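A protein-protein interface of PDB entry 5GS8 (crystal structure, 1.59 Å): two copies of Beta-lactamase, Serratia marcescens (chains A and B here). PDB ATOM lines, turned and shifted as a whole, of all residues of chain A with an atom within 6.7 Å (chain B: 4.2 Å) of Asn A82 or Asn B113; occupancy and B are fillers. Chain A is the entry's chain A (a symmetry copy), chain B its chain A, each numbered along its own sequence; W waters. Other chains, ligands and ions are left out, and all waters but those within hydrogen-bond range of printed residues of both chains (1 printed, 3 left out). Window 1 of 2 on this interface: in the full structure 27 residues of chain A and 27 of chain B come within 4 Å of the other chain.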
ATOM      1  N   GLN A  80     -25.499  28.376   4.209  1.00  0.00           N
ATOM      2  CA  GLN A  80     -25.966  26.990   4.246  1.00  0.00           C
ATOM      3  C   GLN A  80     -26.798  26.740   5.472  1.00  0.00           C
ATOM      4  O   GLN A  80     -26.500  27.238   6.549  1.00  0.00           O
ATOM      5  CB  GLN A  80     -24.791  26.049   4.184  1.00  0.00           C
ATOM      6  CG  GLN A  80     -24.029  26.232   2.873  1.00  0.00           C
ATOM      7  CD  GLN A  80     -22.934  25.186   2.658  1.00  0.00           C
ATOM      8  OE1 GLN A  80     -22.057  24.978   3.517  1.00  0.00           O
ATOM      9  NE2 GLN A  80     -22.983  24.510   1.504  1.00  0.00           N
ATOM     10  N   PRO A  81     -27.817  25.872   5.331  1.00  0.00           N
ATOM     11  CA  PRO A  81     -28.621  25.402   6.450  1.00  0.00           C
ATOM     12  C   PRO A  81     -27.952  24.286   7.250  1.00  0.00           C
ATOM     13  O   PRO A  81     -26.974  23.672   6.813  1.00  0.00           O
ATOM     14  CB  PRO A  81     -29.876  24.876   5.742  1.00  0.00           C
ATOM     15  CG  PRO A  81     -29.284  24.205   4.556  1.00  0.00           C
ATOM     16  CD  PRO A  81     -28.213  25.195   4.085  1.00  0.00           C
ATOM     17  N   ASN A  82     -28.515  24.019   8.433  1.00  0.00           N
ATOM     18  CA  ASN A  82     -28.049  22.945   9.316  1.00  0.00           C
ATOM     19  C   ASN A  82     -26.565  23.035   9.547  1.00  0.00           C
ATOM     20  O   ASN A  82     -25.843  22.054   9.507  1.00  0.00           O
ATOM     21  CB  ASN A  82     -28.453  21.553   8.770  1.00  0.00           C
ATOM     22  CG  ASN A  82     -28.485  20.452   9.831  1.00  0.00           C
ATOM     23  OD1 ASN A  82     -28.866  19.303   9.530  1.00  0.00           O
ATOM     24  ND2 ASN A  82     -28.143  20.773  11.042  1.00  0.00           N
ATOM     25  N   THR A  83     -26.122  24.264   9.799  1.00  0.00           N
ATOM     26  CA  THR A  83     -24.782  24.529  10.289  1.00  0.00           C
ATOM     27  C   THR A  83     -24.883  25.687  11.272  1.00  0.00           C
ATOM     28  O   THR A  83     -25.764  26.537  11.125  1.00  0.00           O
ATOM     29  CB  THR A  83     -23.788  24.813   9.131  1.00  0.00           C
ATOM     30  OG1 THR A  83     -22.448  24.776   9.627  1.00  0.00           O
ATOM     31  CG2 THR A  83     -24.032  26.171   8.457  1.00  0.00           C
ATOM     32  N   TRP A  84     -23.989  25.748  12.250  1.00  0.00           N
ATOM     33  CA  TRP A  84     -24.013  26.847  13.205  1.00  0.00           C
ATOM     34  C   TRP A  84     -23.793  28.168  12.462  1.00  0.00           C
ATOM     35  O   TRP A  84     -22.744  28.368  11.823  1.00  0.00           O
ATOM     36  CB  TRP A  84     -22.912  26.640  14.237  1.00  0.00           C
ATOM     37  CG  TRP A  84     -22.622  27.837  15.076  1.00  0.00           C
ATOM     38  CD1 TRP A  84     -21.576  28.691  14.906  1.00  0.00           C
ATOM     39  CD2 TRP A  84     -23.360  28.341  16.207  1.00  0.00           C
ATOM     40  NE1 TRP A  84     -21.636  29.713  15.819  1.00  0.00           N
ATOM     41  CE2 TRP A  84     -22.698  29.482  16.661  1.00  0.00           C
ATOM     42  CE3 TRP A  84     -24.504  27.923  16.895  1.00  0.00           C
ATOM     43  CZ2 TRP A  84     -23.179  30.261  17.711  1.00  0.00           C
ATOM     44  CZ3 TRP A  84     -24.981  28.728  17.930  1.00  0.00           C
ATOM     45  CH2 TRP A  84     -24.246  29.793  18.399  1.00  0.00           C
ATOM     46  N   LYS A  88     -27.099  33.471   9.408  1.00  0.00           N
ATOM     47  CA  LYS A  88     -28.220  32.946   8.645  1.00  0.00           C
ATOM     48  C   LYS A  88     -29.534  33.147   9.384  1.00  0.00           C
ATOM     49  O   LYS A  88     -30.524  33.491   8.780  1.00  0.00           O
ATOM     50  CB  LYS A  88     -28.011  31.468   8.271  1.00  0.00           C
ATOM     51  CG  LYS A  88     -29.180  30.806   7.530  1.00  0.00           C
ATOM     52  CD  LYS A  88     -28.949  29.314   7.332  1.00  0.00           C
ATOM     53  CE  LYS A  88     -30.239  28.554   7.014  1.00  0.00           C
ATOM     54  NZ  LYS A  88     -30.947  28.130   8.275  1.00  0.00           N
ATOM     55  N   HIS A 151     -17.514  19.622   7.225  1.00  0.00           N
ATOM     56  CA  HIS A 151     -18.813  19.053   7.466  1.00  0.00           C
ATOM     57  C   HIS A 151     -19.106  17.844   6.589  1.00  0.00           C
ATOM     58  O   HIS A 151     -19.997  17.057   6.925  1.00  0.00           O
ATOM     59  CB  HIS A 151     -19.923  20.103   7.305  1.00  0.00           C
ATOM     60  CG  HIS A 151     -20.097  20.989   8.500  1.00  0.00           C
ATOM     61  ND1 HIS A 151     -19.183  21.967   8.815  1.00  0.00           N
ATOM     62  CD2 HIS A 151     -21.153  21.177   9.323  1.00  0.00           C
ATOM     63  CE1 HIS A 151     -19.617  22.647   9.869  1.00  0.00           C
ATOM     64  NE2 HIS A 151     -20.798  22.164  10.211  1.00  0.00           N
ATOM     65  N   GLN B  46     -34.993  14.955   7.943  1.00  0.00           N
ATOM     66  CA  GLN B  46     -34.206  15.967   8.770  1.00  0.00           C
ATOM     67  C   GLN B  46     -35.134  16.792   9.661  1.00  0.00           C
ATOM     68  O   GLN B  46     -35.998  16.209  10.311  1.00  0.00           O
ATOM     69  CB  GLN B  46     -33.310  16.817   7.879  1.00  0.00           C
ATOM     70  CG  GLN B  46     -32.102  16.043   7.377  1.00  0.00           C
ATOM     71  CD  GLN B  46     -30.999  15.902   8.390  1.00  0.00           C
ATOM     72  OE1 GLN B  46     -30.999  16.533   9.457  1.00  0.00           O
ATOM     73  NE2 GLN B  46     -30.043  15.008   8.089  1.00  0.00           N
ATOM     74  N   LYS B  50     -39.477  17.920  13.333  1.00  0.00           N
ATOM     75  CA  LYS B  50     -39.727  18.802  14.482  1.00  0.00           C
ATOM     76  C   LYS B  50     -41.202  19.197  14.536  1.00  0.00           C
ATOM     77  O   LYS B  50     -41.691  19.571  15.600  1.00  0.00           O
ATOM     78  CB  LYS B  50     -38.777  20.006  14.439  1.00  0.00           C
ATOM     79  CG  LYS B  50     -37.303  19.610  14.687  1.00  0.00           C
ATOM     80  CD  LYS B  50     -36.287  20.667  14.280  1.00  0.00           C
ATOM     81  CE  LYS B  50     -34.854  20.135  14.381  1.00  0.00           C
ATOM     82  NZ  LYS B  50     -33.874  21.032  13.759  1.00  0.00           N
ATOM     83  N   THR B  83     -23.590  23.284  16.031  1.00  0.00           N
ATOM     84  CA  THR B  83     -24.835  22.796  15.467  1.00  0.00           C
ATOM     85  C   THR B  83     -25.743  24.001  15.265  1.00  0.00           C
ATOM     86  O   THR B  83     -25.639  24.975  16.014  1.00  0.00           O
ATOM     87  CB  THR B  83     -25.484  21.702  16.358  1.00  0.00           C
ATOM     88  OG1 THR B  83     -26.530  21.051  15.634  1.00  0.00           O
ATOM     89  CG2 THR B  83     -26.059  22.264  17.666  1.00  0.00           C
ATOM     90  N   TRP B  84     -26.637  23.945  14.288  1.00  0.00           N
ATOM     91  CA  TRP B  84     -27.555  25.054  14.063  1.00  0.00           C
ATOM     92  C   TRP B  84     -28.423  25.253  15.309  1.00  0.00           C
ATOM     93  O   TRP B  84     -29.169  24.343  15.713  1.00  0.00           O
ATOM     94  CB  TRP B  84     -28.434  24.740  12.859  1.00  0.00           C
ATOM     95  CG  TRP B  84     -29.617  25.636  12.711  1.00  0.00           C
ATOM     96  CD1 TRP B  84     -30.895  25.327  13.062  1.00  0.00           C
ATOM     97  CD2 TRP B  84     -29.666  26.979  12.191  1.00  0.00           C
ATOM     98  NE1 TRP B  84     -31.726  26.396  12.839  1.00  0.00           N
ATOM     99  CE2 TRP B  84     -30.995  27.401  12.253  1.00  0.00           C
ATOM    100  CE3 TRP B  84     -28.719  27.857  11.655  1.00  0.00           C
ATOM    101  CZ2 TRP B  84     -31.393  28.684  11.885  1.00  0.00           C
ATOM    102  CZ3 TRP B  84     -29.134  29.144  11.312  1.00  0.00           C
ATOM    103  CH2 TRP B  84     -30.467  29.484  11.307  1.00  0.00           C
ATOM    104  N   SER B 111     -36.114  26.144  13.602  1.00  0.00           N
ATOM    105  CA  SER B 111     -35.472  24.840  13.395  1.00  0.00           C
ATOM    106  C   SER B 111     -34.333  24.541  14.366  1.00  0.00           C
ATOM    107  O   SER B 111     -33.397  23.783  14.043  1.00  0.00           O
ATOM    108  CB  SER B 111     -35.009  24.692  11.944  1.00  0.00           C
ATOM    109  OG  SER B 111     -35.036  23.317  11.596  1.00  0.00           O
ATOM    110  N   ASP B 112     -34.407  25.022  15.599  1.00  0.00           N
ATOM    111  CA  ASP B 112     -33.312  24.817  16.526  1.00  0.00           C
ATOM    112  C   ASP B 112     -32.984  23.353  16.756  1.00  0.00           C
ATOM    113  O   ASP B 112     -33.844  22.564  17.145  1.00  0.00           O
ATOM    114  CB  ASP B 112     -33.605  25.503  17.857  1.00  0.00           C
ATOM    115  CG  ASP B 112     -32.353  25.762  18.628  1.00  0.00           C
ATOM    116  OD1 ASP B 112     -31.813  24.809  19.201  1.00  0.00           O
ATOM    117  OD2 ASP B 112     -31.853  26.882  18.597  1.00  0.00           O
ATOM    118  N   ASN B 113     -31.723  22.979  16.598  1.00  0.00           N
ATOM    119  CA  ASN B 113     -31.333  21.565  16.779  1.00  0.00           C
ATOM    120  C   ASN B 113     -31.255  21.200  18.275  1.00  0.00           C
ATOM    121  O   ASN B 113     -31.565  20.078  18.673  1.00  0.00           O
ATOM    122  CB  ASN B 113     -29.974  21.278  16.131  1.00  0.00           C
ATOM    123  CG  ASN B 113     -30.053  21.158  14.623  1.00  0.00           C
ATOM    124  OD1 ASN B 113     -31.134  21.092  14.039  1.00  0.00           O
ATOM    125  ND2 ASN B 113     -28.899  21.186  13.969  1.00  0.00           N
ATOM    126  N   ASN B 114     -30.813  22.150  19.099  1.00  0.00           N
ATOM    127  CA  ASN B 114     -30.733  21.891  20.544  1.00  0.00           C
ATOM    128  C   ASN B 114     -32.134  21.908  21.174  1.00  0.00           C
ATOM    129  O   ASN B 114     -32.444  21.053  22.016  1.00  0.00           O
ATOM    130  CB  ASN B 114     -29.829  22.921  21.231  1.00  0.00           C
ATOM    131  CG  ASN B 114     -28.384  22.691  20.928  1.00  0.00           C
ATOM    132  OD1 ASN B 114     -27.944  21.558  20.909  1.00  0.00           O
ATOM    133  ND2 ASN B 114     -27.650  23.757  20.618  1.00  0.00           N
ATOM    134  N   GLY B 115     -32.983  22.836  20.757  1.00  0.00           N
ATOM    135  CA  GLY B 115     -34.381  22.825  21.226  1.00  0.00           C
ATOM    136  C   GLY B 115     -35.048  21.505  20.934  1.00  0.00           C
ATOM    137  O   GLY B 115     -35.758  20.940  21.762  1.00  0.00           O
ATOM    138  N   CYS B 116     -34.810  20.977  19.747  1.00  0.00           N
ATOM    139  CA  CYS B 116     -35.368  19.704  19.357  1.00  0.00           C
ATOM    140  C   CYS B 116     -34.993  18.609  20.369  1.00  0.00           C
ATOM    141  O   CYS B 116     -35.855  17.916  20.872  1.00  0.00           O
ATOM    142  CB  CYS B 116     -34.838  19.366  17.970  1.00  0.00           C
ATOM    143  SG  CYS B 116     -35.219  17.712  17.358  1.00  0.00           S
ATOM    144  N   ASP B 117     -33.721  18.513  20.702  1.00  0.00           N
ATOM    145  CA  ASP B 117     -33.318  17.463  21.571  1.00  0.00           C
ATOM    146  C   ASP B 117     -33.752  17.678  22.995  1.00  0.00           C
ATOM    147  O   ASP B 117     -34.039  16.698  23.694  1.00  0.00           O
ATOM    148  CB  ASP B 117     -31.824  17.214  21.445  1.00  0.00           C
ATOM    149  CG  ASP B 117     -31.463  16.546  20.096  1.00  0.00           C
ATOM    150  OD1 ASP B 117     -32.373  16.285  19.232  1.00  0.00           O
ATOM    151  OD2 ASP B 117     -30.245  16.380  19.869  1.00  0.00           O
ATOM    152  N   GLU B 147     -31.370  14.902  16.960  1.00  0.00           N
ATOM    153  CA  GLU B 147     -30.461  15.696  16.137  1.00  0.00           C
ATOM    154  C   GLU B 147     -29.031  15.306  16.511  1.00  0.00           C
ATOM    155  O   GLU B 147     -28.195  15.118  15.628  1.00  0.00           O
ATOM    156  CB  GLU B 147     -30.668  17.198  16.321  1.00  0.00           C
ATOM    157  CG  GLU B 147     -31.829  17.707  15.497  1.00  0.00           C
ATOM    158  CD  GLU B 147     -31.510  17.898  14.018  1.00  0.00           C
ATOM    159  OE1 GLU B 147     -30.341  17.672  13.613  1.00  0.00           O
ATOM    160  OE2 GLU B 147     -32.434  18.236  13.196  1.00  0.00           O
ATOM    161  N   HIS B 151     -26.146  13.732  13.914  1.00  0.00           N
ATOM    162  CA  HIS B 151     -24.890  14.400  13.706  1.00  0.00           C
ATOM    163  C   HIS B 151     -23.689  13.480  13.879  1.00  0.00           C
ATOM    164  O   HIS B 151     -22.602  13.810  13.392  1.00  0.00           O
ATOM    165  CB  HIS B 151     -24.751  15.627  14.619  1.00  0.00           C
ATOM    166  CG  HIS B 151     -25.472  16.841  14.118  1.00  0.00           C
ATOM    167  ND1 HIS B 151     -26.843  16.935  14.158  1.00  0.00           N
ATOM    168  CD2 HIS B 151     -25.017  18.063  13.761  1.00  0.00           C
ATOM    169  CE1 HIS B 151     -27.210  18.135  13.725  1.00  0.00           C
ATOM    170  NE2 HIS B 151     -26.118  18.825  13.451  1.00  0.00           N
ATOM    171  N   SER B 218     -33.167  20.008   6.289  1.00  0.00           N
ATOM    172  CA  SER B 218     -31.935  20.100   5.456  1.00  0.00           C
ATOM    173  C   SER B 218     -30.853  19.203   6.051  1.00  0.00           C
ATOM    174  O   SER B 218     -30.601  19.242   7.261  1.00  0.00           O
ATOM    175  CB  SER B 218     -31.397  21.501   5.414  1.00  0.00           C
ATOM    176  OG  SER B 218     -32.384  22.449   5.063  1.00  0.00           O
HETATM  177  O   HOH W   1     -31.156  21.665  11.194  1.00  0.00           O
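The side-chain amide oxygen of Asn B113 lies within hydrogen-bond range of the side-chain amino group of Lys B50 (2.8 Å). The side-chain hydroxyl of Thr B83 is in hydrogen-bond range of the side-chain amide nitrogen of Asn B113. The indole nitrogen (NE1) of Trp B84 sits close to the backbone carbonyl oxygen (O) of Ser B111 (3.3 Å). The backbone NH (N) of Asn B113 sits at hydrogen-bond distance from the backbone carbonyl oxygen (O) of Trp B84 (3.0 Å). The backbone carbonyl oxygen of Glu B147 is in hydrogen-bond range of a ring nitrogen (ND1) of His B151, 2.7 Å away. NE2 of His A151 sits at hydrogen-bond distance from OG1 of Thr A83.
Water W1 bridges the side-chain amide oxygen of Asn B113 and the side-chain amide nitrogen of Asn A82.
The side-chain amide oxygen (OD1) of Asn A82 sits close to the side-chain amide oxygen (OE1) of Gln B46, 3.5 Å away. The side-chain amide nitrogen (ND2) of Asn B113 lies close to the side-chain amide nitrogen (ND2) of Asn A82 (3.1 Å). O of Ser B218 sits close to OD1 of Asn A82, at 2.9 Å.
Hydrophobic or aromatic side chains of chain A within 4 Å of the printed part of chain B: Pro A81 and Trp A84. Along chain A the printed residues that touch a printed residue of chain B span positions 81 to 88. Hydrophobic or aromatic side chains of chain B within 4 Å of the printed part of chain A: Trp B84 and His B151. Along chain B the printed residues that touch a printed residue of chain A span positions 46 to 218. Among the printed residues, 10 pairs touch across the chains. Among the printed residues, no Asp or Glu carboxylate lies within 4 Å of a Lys or Arg side-chain nitrogen of the other chain.
Thr A83 touches Trp B84, and with the chains exchanged Trp A84 touches Thr B83. Trp A84 touches its own counterpart, Trp B84. 3 positions are printed for both chains. Of the 10 pairs that touch across the chains among the printed residues, 3 have their exchanged pair printed and touching as well.
Pro A81 touches Ser B218. CB of Trp B84 touches CA of Asn A82, at 3.99 Å. Asn A82 touches His B151 (ND2 to NE2, 3.7 Å). CE3 of Trp B84 touches O of Thr A83, at 3.3 Å. Thr B83 touches Trp A84. Trp B84 touches Trp A84 (N to N, 3.8 Å). Trp B84 touches Lys A88 (CH2 to NZ, 3.4 Å).
Printed residues of chain B within 4 Å of Pro A81: Ser B218 (3.5 Å). Of the printed residues of chain B, Asn A82 touches Gln B46, Trp B84, Asn B113, His B151 and Ser B218. Printed residues of chain B within 4 Å of Thr A83: Trp B84. Of the printed residues of chain B, Trp A84 touches Thr B83 (3.3 Å) and Trp B84 (3.8 Å). His A151 touches none of the printed residues of chain B. Of the printed residues of chain A, Thr B83 touches Trp A84. Of the printed residues of chain A, Trp B84 touches Asn A82, Thr A83, Trp A84 and Lys A88. Of chain A, only Asn A82 (3.1 Å) comes within 4 Å of Asn B113. Asn B114 touches none of the printed residues of chain A.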
